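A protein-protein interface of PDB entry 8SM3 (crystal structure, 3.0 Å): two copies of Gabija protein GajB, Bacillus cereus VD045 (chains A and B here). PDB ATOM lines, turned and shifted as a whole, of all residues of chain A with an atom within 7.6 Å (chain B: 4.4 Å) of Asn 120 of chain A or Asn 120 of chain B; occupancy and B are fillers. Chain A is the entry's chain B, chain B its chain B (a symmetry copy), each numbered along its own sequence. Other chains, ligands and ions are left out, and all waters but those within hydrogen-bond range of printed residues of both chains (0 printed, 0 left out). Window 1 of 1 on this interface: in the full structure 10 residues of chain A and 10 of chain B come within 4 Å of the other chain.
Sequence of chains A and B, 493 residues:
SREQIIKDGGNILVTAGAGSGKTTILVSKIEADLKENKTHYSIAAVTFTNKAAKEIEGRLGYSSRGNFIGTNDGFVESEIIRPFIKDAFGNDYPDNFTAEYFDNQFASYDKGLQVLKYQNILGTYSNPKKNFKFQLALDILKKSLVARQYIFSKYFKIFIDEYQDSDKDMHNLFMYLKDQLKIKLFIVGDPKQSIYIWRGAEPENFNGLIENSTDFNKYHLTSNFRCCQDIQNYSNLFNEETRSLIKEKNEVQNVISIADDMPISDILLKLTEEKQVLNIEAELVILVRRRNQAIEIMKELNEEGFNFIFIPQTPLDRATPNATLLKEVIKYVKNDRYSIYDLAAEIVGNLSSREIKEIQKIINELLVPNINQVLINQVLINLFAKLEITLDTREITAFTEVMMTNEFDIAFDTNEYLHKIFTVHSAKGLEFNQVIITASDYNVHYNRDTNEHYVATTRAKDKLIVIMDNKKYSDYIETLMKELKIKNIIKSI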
ATOM      1  N   ASP A  92     -28.586  14.600   9.089  1.00  0.00           N
ATOM      2  CA  ASP A  92     -29.468  15.212  10.077  1.00  0.00           C
ATOM      3  C   ASP A  92     -28.945  16.565  10.543  1.00  0.00           C
ATOM      4  O   ASP A  92     -29.737  17.450  10.885  1.00  0.00           O
ATOM      5  CB  ASP A  92     -29.640  14.282  11.276  1.00  0.00           C
ATOM      6  CG  ASP A  92     -30.240  12.945  10.897  1.00  0.00           C
ATOM      7  OD1 ASP A  92     -31.296  12.932  10.229  1.00  0.00           O
ATOM      8  OD2 ASP A  92     -29.650  11.908  11.265  1.00  0.00           O
ATOM      9  N   TYR A  93     -27.628  16.743  10.563  1.00  0.00           N
ATOM     10  CA  TYR A  93     -26.965  17.930  11.087  1.00  0.00           C
ATOM     11  C   TYR A  93     -26.866  19.009  10.012  1.00  0.00           C
ATOM     12  O   TYR A  93     -26.643  18.699   8.838  1.00  0.00           O
ATOM     13  CB  TYR A  93     -25.570  17.581  11.600  1.00  0.00           C
ATOM     14  CG  TYR A  93     -25.582  16.690  12.822  1.00  0.00           C
ATOM     15  CD1 TYR A  93     -25.978  15.361  12.734  1.00  0.00           C
ATOM     16  CD2 TYR A  93     -25.192  17.175  14.065  1.00  0.00           C
ATOM     17  CE1 TYR A  93     -25.994  14.545  13.844  1.00  0.00           C
ATOM     18  CE2 TYR A  93     -25.203  16.362  15.183  1.00  0.00           C
ATOM     19  CZ  TYR A  93     -25.604  15.047  15.066  1.00  0.00           C
ATOM     20  OH  TYR A  93     -25.617  14.232  16.174  1.00  0.00           O
ATOM     21  N   PRO A  94     -27.030  20.273  10.388  1.00  0.00           N
ATOM     22  CA  PRO A  94     -27.018  21.356   9.403  1.00  0.00           C
ATOM     23  C   PRO A  94     -25.631  21.932   9.169  1.00  0.00           C
ATOM     24  O   PRO A  94     -24.751  21.904  10.032  1.00  0.00           O
ATOM     25  CB  PRO A  94     -27.934  22.403  10.050  1.00  0.00           C
ATOM     26  CG  PRO A  94     -27.673  22.229  11.513  1.00  0.00           C
ATOM     27  CD  PRO A  94     -27.399  20.756  11.732  1.00  0.00           C
ATOM     28  N   ASP A  95     -25.447  22.466   7.962  1.00  0.00           N
ATOM     29  CA  ASP A  95     -24.243  23.204   7.611  1.00  0.00           C
ATOM     30  C   ASP A  95     -24.457  24.712   7.588  1.00  0.00           C
ATOM     31  O   ASP A  95     -23.489  25.457   7.409  1.00  0.00           O
ATOM     32  CB  ASP A  95     -23.710  22.739   6.250  1.00  0.00           C
ATOM     33  CG  ASP A  95     -24.804  22.610   5.211  1.00  0.00           C
ATOM     34  OD1 ASP A  95     -25.985  22.817   5.563  1.00  0.00           O
ATOM     35  OD2 ASP A  95     -24.485  22.299   4.044  1.00  0.00           O
ATOM     36  N   ASN A  96     -25.696  25.175   7.761  1.00  0.00           N
ATOM     37  CA  ASN A  96     -26.005  26.592   7.883  1.00  0.00           C
ATOM     38  C   ASN A  96     -26.118  27.033   9.337  1.00  0.00           C
ATOM     39  O   ASN A  96     -26.799  28.023   9.630  1.00  0.00           O
ATOM     40  CB  ASN A  96     -27.294  26.919   7.126  1.00  0.00           C
ATOM     41  CG  ASN A  96     -28.456  26.032   7.536  1.00  0.00           C
ATOM     42  OD1 ASN A  96     -28.399  25.337   8.551  1.00  0.00           O
ATOM     43  ND2 ASN A  96     -29.524  26.055   6.747  1.00  0.00           N
ATOM     44  N   PHE A  97     -25.470  26.314  10.249  1.00  0.00           N
ATOM     45  CA  PHE A  97     -25.577  26.608  11.670  1.00  0.00           C
ATOM     46  C   PHE A  97     -24.956  27.961  11.995  1.00  0.00           C
ATOM     47  O   PHE A  97     -24.081  28.459  11.281  1.00  0.00           O
ATOM     48  CB  PHE A  97     -24.896  25.512  12.490  1.00  0.00           C
ATOM     49  CG  PHE A  97     -23.443  25.313  12.151  1.00  0.00           C
ATOM     50  CD1 PHE A  97     -23.068  24.461  11.126  1.00  0.00           C
ATOM     51  CD2 PHE A  97     -22.454  25.977  12.859  1.00  0.00           C
ATOM     52  CE1 PHE A  97     -21.736  24.276  10.811  1.00  0.00           C
ATOM     53  CE2 PHE A  97     -21.119  25.796  12.548  1.00  0.00           C
ATOM     54  CZ  PHE A  97     -20.761  24.944  11.522  1.00  0.00           C
ATOM     55  N   THR A  98     -25.420  28.555  13.091  1.00  0.00           N
ATOM     56  CA  THR A  98     -24.909  29.828  13.581  1.00  0.00           C
ATOM     57  C   THR A  98     -24.369  29.629  14.989  1.00  0.00           C
ATOM     58  O   THR A  98     -25.095  29.163  15.873  1.00  0.00           O
ATOM     59  CB  THR A  98     -26.000  30.903  13.580  1.00  0.00           C
ATOM     60  OG1 THR A  98     -26.658  30.918  12.307  1.00  0.00           O
ATOM     61  CG2 THR A  98     -25.391  32.270  13.846  1.00  0.00           C
ATOM     62  N   ALA A  99     -23.103  29.979  15.193  1.00  0.00           N
ATOM     63  CA  ALA A  99     -22.440  29.770  16.473  1.00  0.00           C
ATOM     64  C   ALA A  99     -22.605  31.012  17.341  1.00  0.00           C
ATOM     65  O   ALA A  99     -22.237  32.119  16.929  1.00  0.00           O
ATOM     66  CB  ALA A  99     -20.961  29.445  16.274  1.00  0.00           C
ATOM     67  N   LEU A 113     -24.568  18.374  21.047  1.00  0.00           N
ATOM     68  CA  LEU A 113     -24.910  17.846  19.730  1.00  0.00           C
ATOM     69  C   LEU A 113     -26.387  18.055  19.423  1.00  0.00           C
ATOM     70  O   LEU A 113     -26.759  18.313  18.272  1.00  0.00           O
ATOM     71  CB  LEU A 113     -24.551  16.361  19.649  1.00  0.00           C
ATOM     72  CG  LEU A 113     -23.087  15.988  19.885  1.00  0.00           C
ATOM     73  CD1 LEU A 113     -22.893  14.487  19.754  1.00  0.00           C
ATOM     74  CD2 LEU A 113     -22.176  16.737  18.924  1.00  0.00           C
ATOM     75  N   GLN A 114     -27.243  17.953  20.442  1.00  0.00           N
ATOM     76  CA  GLN A 114     -28.672  18.150  20.227  1.00  0.00           C
ATOM     77  C   GLN A 114     -29.002  19.613  19.962  1.00  0.00           C
ATOM     78  O   GLN A 114     -29.931  19.910  19.202  1.00  0.00           O
ATOM     79  CB  GLN A 114     -29.457  17.634  21.433  1.00  0.00           C
ATOM     80  CG  GLN A 114     -28.921  16.327  21.995  1.00  0.00           C
ATOM     81  CD  GLN A 114     -29.993  15.491  22.664  1.00  0.00           C
ATOM     82  OE1 GLN A 114     -30.925  15.019  22.012  1.00  0.00           O
ATOM     83  NE2 GLN A 114     -29.868  15.303  23.973  1.00  0.00           N
ATOM     84  N   VAL A 115     -28.261  20.535  20.577  1.00  0.00           N
ATOM     85  CA  VAL A 115     -28.460  21.954  20.295  1.00  0.00           C
ATOM     86  C   VAL A 115     -28.076  22.260  18.854  1.00  0.00           C
ATOM     87  O   VAL A 115     -28.691  23.105  18.193  1.00  0.00           O
ATOM     88  CB  VAL A 115     -27.656  22.812  21.287  1.00  0.00           C
ATOM     89  CG1 VAL A 115     -28.148  24.244  21.266  1.00  0.00           C
ATOM     90  CG2 VAL A 115     -27.752  22.229  22.685  1.00  0.00           C
ATOM     91  N   LEU A 116     -27.057  21.573  18.345  1.00  0.00           N
ATOM     92  CA  LEU A 116     -26.641  21.771  16.965  1.00  0.00           C
ATOM     93  C   LEU A 116     -27.558  21.035  15.996  1.00  0.00           C
ATOM     94  O   LEU A 116     -27.807  21.515  14.885  1.00  0.00           O
ATOM     95  CB  LEU A 116     -25.193  21.314  16.806  1.00  0.00           C
ATOM     96  CG  LEU A 116     -24.537  21.301  15.431  1.00  0.00           C
ATOM     97  CD1 LEU A 116     -24.645  22.656  14.755  1.00  0.00           C
ATOM     98  CD2 LEU A 116     -23.089  20.907  15.620  1.00  0.00           C
ATOM     99  N   LYS A 117     -28.083  19.882  16.409  1.00  0.00           N
ATOM    100  CA  LYS A 117     -28.914  19.075  15.524  1.00  0.00           C
ATOM    101  C   LYS A 117     -30.335  19.622  15.441  1.00  0.00           C
ATOM    102  O   LYS A 117     -30.912  19.706  14.351  1.00  0.00           O
ATOM    103  CB  LYS A 117     -28.919  17.622  16.004  1.00  0.00           C
ATOM    104  CG  LYS A 117     -29.752  16.667  15.164  1.00  0.00           C
ATOM    105  CD  LYS A 117     -29.552  15.232  15.633  1.00  0.00           C
ATOM    106  CE  LYS A 117     -30.362  14.251  14.802  1.00  0.00           C
ATOM    107  NZ  LYS A 117     -30.049  12.836  15.143  1.00  0.00           N
ATOM    108  N   TYR A 118     -30.911  20.008  16.579  1.00  0.00           N
ATOM    109  CA  TYR A 118     -32.296  20.458  16.636  1.00  0.00           C
ATOM    110  C   TYR A 118     -32.425  21.976  16.688  1.00  0.00           C
ATOM    111  O   TYR A 118     -33.192  22.557  15.916  1.00  0.00           O
ATOM    112  CB  TYR A 118     -32.999  19.828  17.846  1.00  0.00           C
ATOM    113  CG  TYR A 118     -32.907  18.318  17.887  1.00  0.00           C
ATOM    114  CD1 TYR A 118     -33.645  17.534  17.010  1.00  0.00           C
ATOM    115  CD2 TYR A 118     -32.083  17.678  18.803  1.00  0.00           C
ATOM    116  CE1 TYR A 118     -33.563  16.153  17.044  1.00  0.00           C
ATOM    117  CE2 TYR A 118     -31.995  16.297  18.844  1.00  0.00           C
ATOM    118  CZ  TYR A 118     -32.737  15.541  17.964  1.00  0.00           C
ATOM    119  OH  TYR A 118     -32.651  14.168  18.003  1.00  0.00           O
ATOM    120  N   GLN A 119     -31.690  22.633  17.585  1.00  0.00           N
ATOM    121  CA  GLN A 119     -31.772  24.083  17.720  1.00  0.00           C
ATOM    122  C   GLN A 119     -30.907  24.828  16.710  1.00  0.00           C
ATOM    123  O   GLN A 119     -30.951  26.062  16.679  1.00  0.00           O
ATOM    124  CB  GLN A 119     -31.397  24.494  19.147  1.00  0.00           C
ATOM    125  CG  GLN A 119     -32.484  24.182  20.167  1.00  0.00           C
ATOM    126  CD  GLN A 119     -31.975  23.401  21.361  1.00  0.00           C
ATOM    127  OE1 GLN A 119     -31.211  23.916  22.176  1.00  0.00           O
ATOM    128  NE2 GLN A 119     -32.402  22.148  21.473  1.00  0.00           N
ATOM    129  N   ASN A 120     -30.123  24.113  15.900  1.00  0.00           N
ATOM    130  CA  ASN A 120     -29.430  24.685  14.742  1.00  0.00           C
ATOM    131  C   ASN A 120     -28.426  25.767  15.139  1.00  0.00           C
ATOM    132  O   ASN A 120     -28.148  26.687  14.365  1.00  0.00           O
ATOM    133  CB  ASN A 120     -30.437  25.235  13.723  1.00  0.00           C
ATOM    134  CG  ASN A 120     -29.811  25.504  12.365  1.00  0.00           C
ATOM    135  OD1 ASN A 120     -29.825  24.649  11.481  1.00  0.00           O
ATOM    136  ND2 ASN A 120     -29.256  26.699  12.198  1.00  0.00           N
ATOM    137  N   ILE A 121     -27.864  25.681  16.345  1.00  0.00           N
ATOM    138  CA  ILE A 121     -26.852  26.634  16.785  1.00  0.00           C
ATOM    139  C   ILE A 121     -25.707  25.877  17.446  1.00  0.00           C
ATOM    140  O   ILE A 121     -25.870  24.765  17.949  1.00  0.00           O
ATOM    141  CB  ILE A 121     -27.409  27.707  17.751  1.00  0.00           C
ATOM    142  CG1 ILE A 121     -27.808  27.087  19.090  1.00  0.00           C
ATOM    143  CG2 ILE A 121     -28.576  28.459  17.122  1.00  0.00           C
ATOM    144  CD1 ILE A 121     -26.856  27.430  20.215  1.00  0.00           C
ATOM    145  N   LEU A 122     -24.536  26.505  17.443  1.00  0.00           N
ATOM    146  CA  LEU A 122     -23.313  25.940  18.005  1.00  0.00           C
ATOM    147  C   LEU A 122     -22.970  26.699  19.280  1.00  0.00           C
ATOM    148  O   LEU A 122     -22.479  27.832  19.220  1.00  0.00           O
ATOM    149  CB  LEU A 122     -22.176  26.017  16.985  1.00  0.00           C
ATOM    150  CG  LEU A 122     -20.909  25.202  17.245  1.00  0.00           C
ATOM    151  CD1 LEU A 122     -21.247  23.731  17.372  1.00  0.00           C
ATOM    152  CD2 LEU A 122     -19.916  25.423  16.118  1.00  0.00           C
ATOM    153  N   GLY A 123     -23.225  26.069  20.428  1.00  0.00           N
ATOM    154  CA  GLY A 123     -23.026  26.705  21.710  1.00  0.00           C
ATOM    155  C   GLY A 123     -21.715  26.314  22.379  1.00  0.00           C
ATOM    156  O   GLY A 123     -21.133  25.265  22.094  1.00  0.00           O
ATOM    157  N   ARG A 354     -25.162  39.227  15.073  1.00  0.00           N
ATOM    158  CA  ARG A 354     -26.199  39.363  16.088  1.00  0.00           C
ATOM    159  C   ARG A 354     -25.592  39.539  17.475  1.00  0.00           C
ATOM    160  O   ARG A 354     -26.072  40.354  18.270  1.00  0.00           O
ATOM    161  CB  ARG A 354     -27.133  38.152  16.057  1.00  0.00           C
ATOM    162  CG  ARG A 354     -28.201  38.171  17.147  1.00  0.00           C
ATOM    163  CD  ARG A 354     -29.334  37.198  16.857  1.00  0.00           C
ATOM    164  NE  ARG A 354     -28.909  35.805  16.914  1.00  0.00           N
ATOM    165  CZ  ARG A 354     -29.716  34.770  16.721  1.00  0.00           C
ATOM    166  NH1 ARG A 354     -31.001  34.937  16.453  1.00  0.00           N
ATOM    167  NH2 ARG A 354     -29.221  33.538  16.799  1.00  0.00           N
ATOM    168  N   PRO B  94     -33.462  35.010  11.491  1.00  0.00           N
ATOM    169  CA  PRO B  94     -32.679  34.431  10.398  1.00  0.00           C
ATOM    170  C   PRO B  94     -33.490  34.220   9.130  1.00  0.00           C
ATOM    171  O   PRO B  94     -34.707  34.034   9.151  1.00  0.00           O
ATOM    172  CB  PRO B  94     -32.237  33.085  10.987  1.00  0.00           C
ATOM    173  CG  PRO B  94     -33.391  32.695  11.854  1.00  0.00           C
ATOM    174  CD  PRO B  94     -33.964  33.978  12.415  1.00  0.00           C
ATOM    175  N   ASN B  96     -32.044  31.848   6.943  1.00  0.00           N
ATOM    176  CA  ASN B  96     -31.669  30.472   6.649  1.00  0.00           C
ATOM    177  C   ASN B  96     -32.441  29.472   7.502  1.00  0.00           C
ATOM    178  O   ASN B  96     -31.961  28.356   7.731  1.00  0.00           O
ATOM    179  CB  ASN B  96     -30.163  30.282   6.839  1.00  0.00           C
ATOM    180  CG  ASN B  96     -29.683  30.739   8.207  1.00  0.00           C
ATOM    181  OD1 ASN B  96     -30.479  30.967   9.117  1.00  0.00           O
ATOM    182  ND2 ASN B  96     -28.369  30.871   8.357  1.00  0.00           N
ATOM    183  N   PHE B  97     -33.622  29.855   7.980  1.00  0.00           N
ATOM    184  CA  PHE B  97     -34.401  29.002   8.865  1.00  0.00           C
ATOM    185  C   PHE B  97     -34.868  27.745   8.140  1.00  0.00           C
ATOM    186  O   PHE B  97     -34.998  27.718   6.913  1.00  0.00           O
ATOM    187  CB  PHE B  97     -35.607  29.767   9.411  1.00  0.00           C
ATOM    188  CG  PHE B  97     -36.519  30.307   8.344  1.00  0.00           C
ATOM    189  CD1 PHE B  97     -36.281  31.546   7.772  1.00  0.00           C
ATOM    190  CD2 PHE B  97     -37.615  29.576   7.914  1.00  0.00           C
ATOM    191  CE1 PHE B  97     -37.116  32.044   6.791  1.00  0.00           C
ATOM    192  CE2 PHE B  97     -38.454  30.070   6.932  1.00  0.00           C
ATOM    193  CZ  PHE B  97     -38.204  31.305   6.371  1.00  0.00           C
ATOM    194  N   THR B  98     -35.122  26.697   8.918  1.00  0.00           N
ATOM    195  CA  THR B  98     -35.624  25.430   8.404  1.00  0.00           C
ATOM    196  C   THR B  98     -36.959  25.128   9.068  1.00  0.00           C
ATOM    197  O   THR B  98     -37.046  25.081  10.299  1.00  0.00           O
ATOM    198  CB  THR B  98     -34.634  24.293   8.666  1.00  0.00           C
ATOM    199  OG1 THR B  98     -33.324  24.688   8.240  1.00  0.00           O
ATOM    200  CG2 THR B  98     -35.052  23.046   7.904  1.00  0.00           C
ATOM    201  N   VAL B 115     -38.976  30.490  18.878  1.00  0.00           N
ATOM    202  CA  VAL B 115     -38.427  29.294  18.248  1.00  0.00           C
ATOM    203  C   VAL B 115     -37.753  29.655  16.934  1.00  0.00           C
ATOM    204  O   VAL B 115     -36.738  29.063  16.549  1.00  0.00           O
ATOM    205  CB  VAL B 115     -39.535  28.244  18.047  1.00  0.00           C
ATOM    206  CG1 VAL B 115     -38.927  26.884  17.770  1.00  0.00           C
ATOM    207  CG2 VAL B 115     -40.441  28.194  19.262  1.00  0.00           C
ATOM    208  N   LEU B 116     -38.306  30.637  16.225  1.00  0.00           N
ATOM    209  CA  LEU B 116     -37.710  31.077  14.971  1.00  0.00           C
ATOM    210  C   LEU B 116     -36.515  31.989  15.213  1.00  0.00           C
ATOM    211  O   LEU B 116     -35.546  31.964  14.447  1.00  0.00           O
ATOM    212  CB  LEU B 116     -38.775  31.775  14.129  1.00  0.00           C
ATOM    213  CG  LEU B 116     -38.398  32.442  12.812  1.00  0.00           C
ATOM    214  CD1 LEU B 116     -37.677  31.474  11.891  1.00  0.00           C
ATOM    215  CD2 LEU B 116     -39.674  32.944  12.173  1.00  0.00           C
ATOM    216  N   TYR B 118     -34.510  32.165  18.143  1.00  0.00           N
ATOM    217  CA  TYR B 118     -33.430  31.522  18.882  1.00  0.00           C
ATOM    218  C   TYR B 118     -33.132  30.111  18.387  1.00  0.00           C
ATOM    219  O   TYR B 118     -31.970  29.779  18.134  1.00  0.00           O
ATOM    220  CB  TYR B 118     -33.765  31.496  20.378  1.00  0.00           C
ATOM    221  CG  TYR B 118     -34.095  32.857  20.953  1.00  0.00           C
ATOM    222  CD1 TYR B 118     -33.100  33.803  21.161  1.00  0.00           C
ATOM    223  CD2 TYR B 118     -35.399  33.194  21.291  1.00  0.00           C
ATOM    224  CE1 TYR B 118     -33.395  35.049  21.686  1.00  0.00           C
ATOM    225  CE2 TYR B 118     -35.705  34.437  21.816  1.00  0.00           C
ATOM    226  CZ  TYR B 118     -34.700  35.359  22.012  1.00  0.00           C
ATOM    227  OH  TYR B 118     -35.001  36.596  22.534  1.00  0.00           O
ATOM    228  N   GLN B 119     -34.156  29.271  18.247  1.00  0.00           N
ATOM    229  CA  GLN B 119     -33.957  27.896  17.806  1.00  0.00           C
ATOM    230  C   GLN B 119     -33.853  27.762  16.291  1.00  0.00           C
ATOM    231  O   GLN B 119     -33.610  26.652  15.802  1.00  0.00           O
ATOM    232  CB  GLN B 119     -35.085  27.009  18.341  1.00  0.00           C
ATOM    233  CG  GLN B 119     -34.960  26.714  19.830  1.00  0.00           C
ATOM    234  CD  GLN B 119     -36.225  27.018  20.606  1.00  0.00           C
ATOM    235  OE1 GLN B 119     -37.241  26.342  20.449  1.00  0.00           O
ATOM    236  NE2 GLN B 119     -36.166  28.037  21.455  1.00  0.00           N
ATOM    237  N   ASN B 120     -34.041  28.854  15.545  1.00  0.00           N
ATOM    238  CA  ASN B 120     -33.740  28.909  14.112  1.00  0.00           C
ATOM    239  C   ASN B 120     -34.584  27.928  13.299  1.00  0.00           C
ATOM    240  O   ASN B 120     -34.160  27.451  12.244  1.00  0.00           O
ATOM    241  CB  ASN B 120     -32.246  28.668  13.860  1.00  0.00           C
ATOM    242  CG  ASN B 120     -31.813  29.067  12.461  1.00  0.00           C
ATOM    243  OD1 ASN B 120     -31.372  30.191  12.231  1.00  0.00           O
ATOM    244  ND2 ASN B 120     -31.941  28.140  11.517  1.00  0.00           N
ATOM    245  N   ILE B 121     -35.791  27.607  13.770  1.00  0.00           N
ATOM    246  CA  ILE B 121     -36.688  26.727  13.033  1.00  0.00           C
ATOM    247  C   ILE B 121     -38.090  27.321  13.044  1.00  0.00           C
ATOM    248  O   ILE B 121     -38.458  28.098  13.927  1.00  0.00           O
ATOM    249  CB  ILE B 121     -36.716  25.284  13.593  1.00  0.00           C
ATOM    250  CG1 ILE B 121     -37.361  25.245  14.977  1.00  0.00           C
ATOM    251  CG2 ILE B 121     -35.318  24.679  13.619  1.00  0.00           C
ATOM    252  CD1 ILE B 121     -38.745  24.630  14.976  1.00  0.00           C
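The side-chain amide nitrogen of Asn 96 of chain B sits at hydrogen-bond distance from the backbone carbonyl oxygen of Asn 96 of chain A (3.5 Å). ND2 of Asn 120 of chain B lies close to ND2 of Asn 120 of chain A. The backbone carbonyl oxygen (O) of Gln 119 of chain B lies close to the backbone carbonyl oxygen (O) of Gln 119 of chain A (2.9 Å).
The backbone carbonyl oxygen of Val 115 of chain A sits at hydrogen-bond distance from the backbone NH of Asn 120 of chain A, 2.9 Å away. The side-chain amide oxygen of Asn 96 of chain A sits close to the side-chain amide oxygen of Asn 120 of chain A. The backbone carbonyl oxygen of Val 115 of chain A is in hydrogen-bond range of the backbone NH of Ile 121 of chain A, at 3.3 Å. The backbone carbonyl oxygen (O) of Val 115 of chain B sits at hydrogen-bond distance from the backbone NH (N) of Ile 121 of chain B (3.3 Å). The backbone NH (N) of Leu 116 of chain A lies close to the backbone carbonyl oxygen (O) of Ile 121 of chain A (3.4 Å). N of Asn 120 of chain B sits at hydrogen-bond distance from O of Val 115 of chain B (2.9 Å).
O of Tyr 118 of chain A touches CG2 of Ile 121 of chain B, 3.8 Å away. CG2 of Ile 121 of chain A touches O of Tyr 118 of chain B (3.8 Å).
Asp 92 of chain A touches none of the printed residues of chain B. Asn 120 of chain A touches one residue of chain B. Printed residues of chain B within 4 Å of Ile 121 of chain A: Tyr 118. Of the printed residues of chain A, Asn 96 of chain B touches Asn 96 (3.5 Å). Of the printed residues of chain A, Tyr 118 of chain B touches Ile 121. Printed residues of chain A within 4 Å of Gln 119 of chain B: Gln 119. Of chain A, only Asn 120 (3.1 Å) comes within 4 Å of Asn 120 of chain B. Of the printed residues of chain A, Ile 121 of chain B touches Tyr 118. The nearest residue of chain B that does not touch Asn 120 of chain A is Gln 119 of chain B (4.05 Å). The nearest residue of chain A that does not touch Asn 120 of chain B is Gln 119 of chain A (4.1 Å).
Of the 20 printed residues of chain A, 5 touch a printed residue of chain B. Printed residues of chain A that touch a printed residue of chain B: Asn 96, Tyr 118, Gln 119, Asn 120 and Ile 121. Hydrophobic or aromatic side chains of chain A that line the printed part of chain B: Ile 121. Printed residues of chain B that touch a printed residue of chain A: Asn 96, Tyr 118, Gln 119, Asn 120 and Ile 121. Hydrophobic or aromatic side chains of chain B that line the printed part of chain A: Ile 121. Among the printed residues, 5 pairs touch across the chains.
Asn 96 of chain B touches its own counterpart, Asn 96 of chain A. Tyr 118 of chain A touches Ile 121 of chain B, and with the chains exchanged Ile 121 of chain A touches Tyr 118 of chain B. Gln 119 of chain B touches its own counterpart, Gln 119 of chain A. Asn 120 of chain B touches its own counterpart, Asn 120 of chain A. Positions printed for both chains: 94, 96, 97, 98, 115, 116, 118, 119, 120 and 121. Of the 5 pairs that touch across the chains among the printed residues, 5 have their exchanged pair printed and touching as well.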
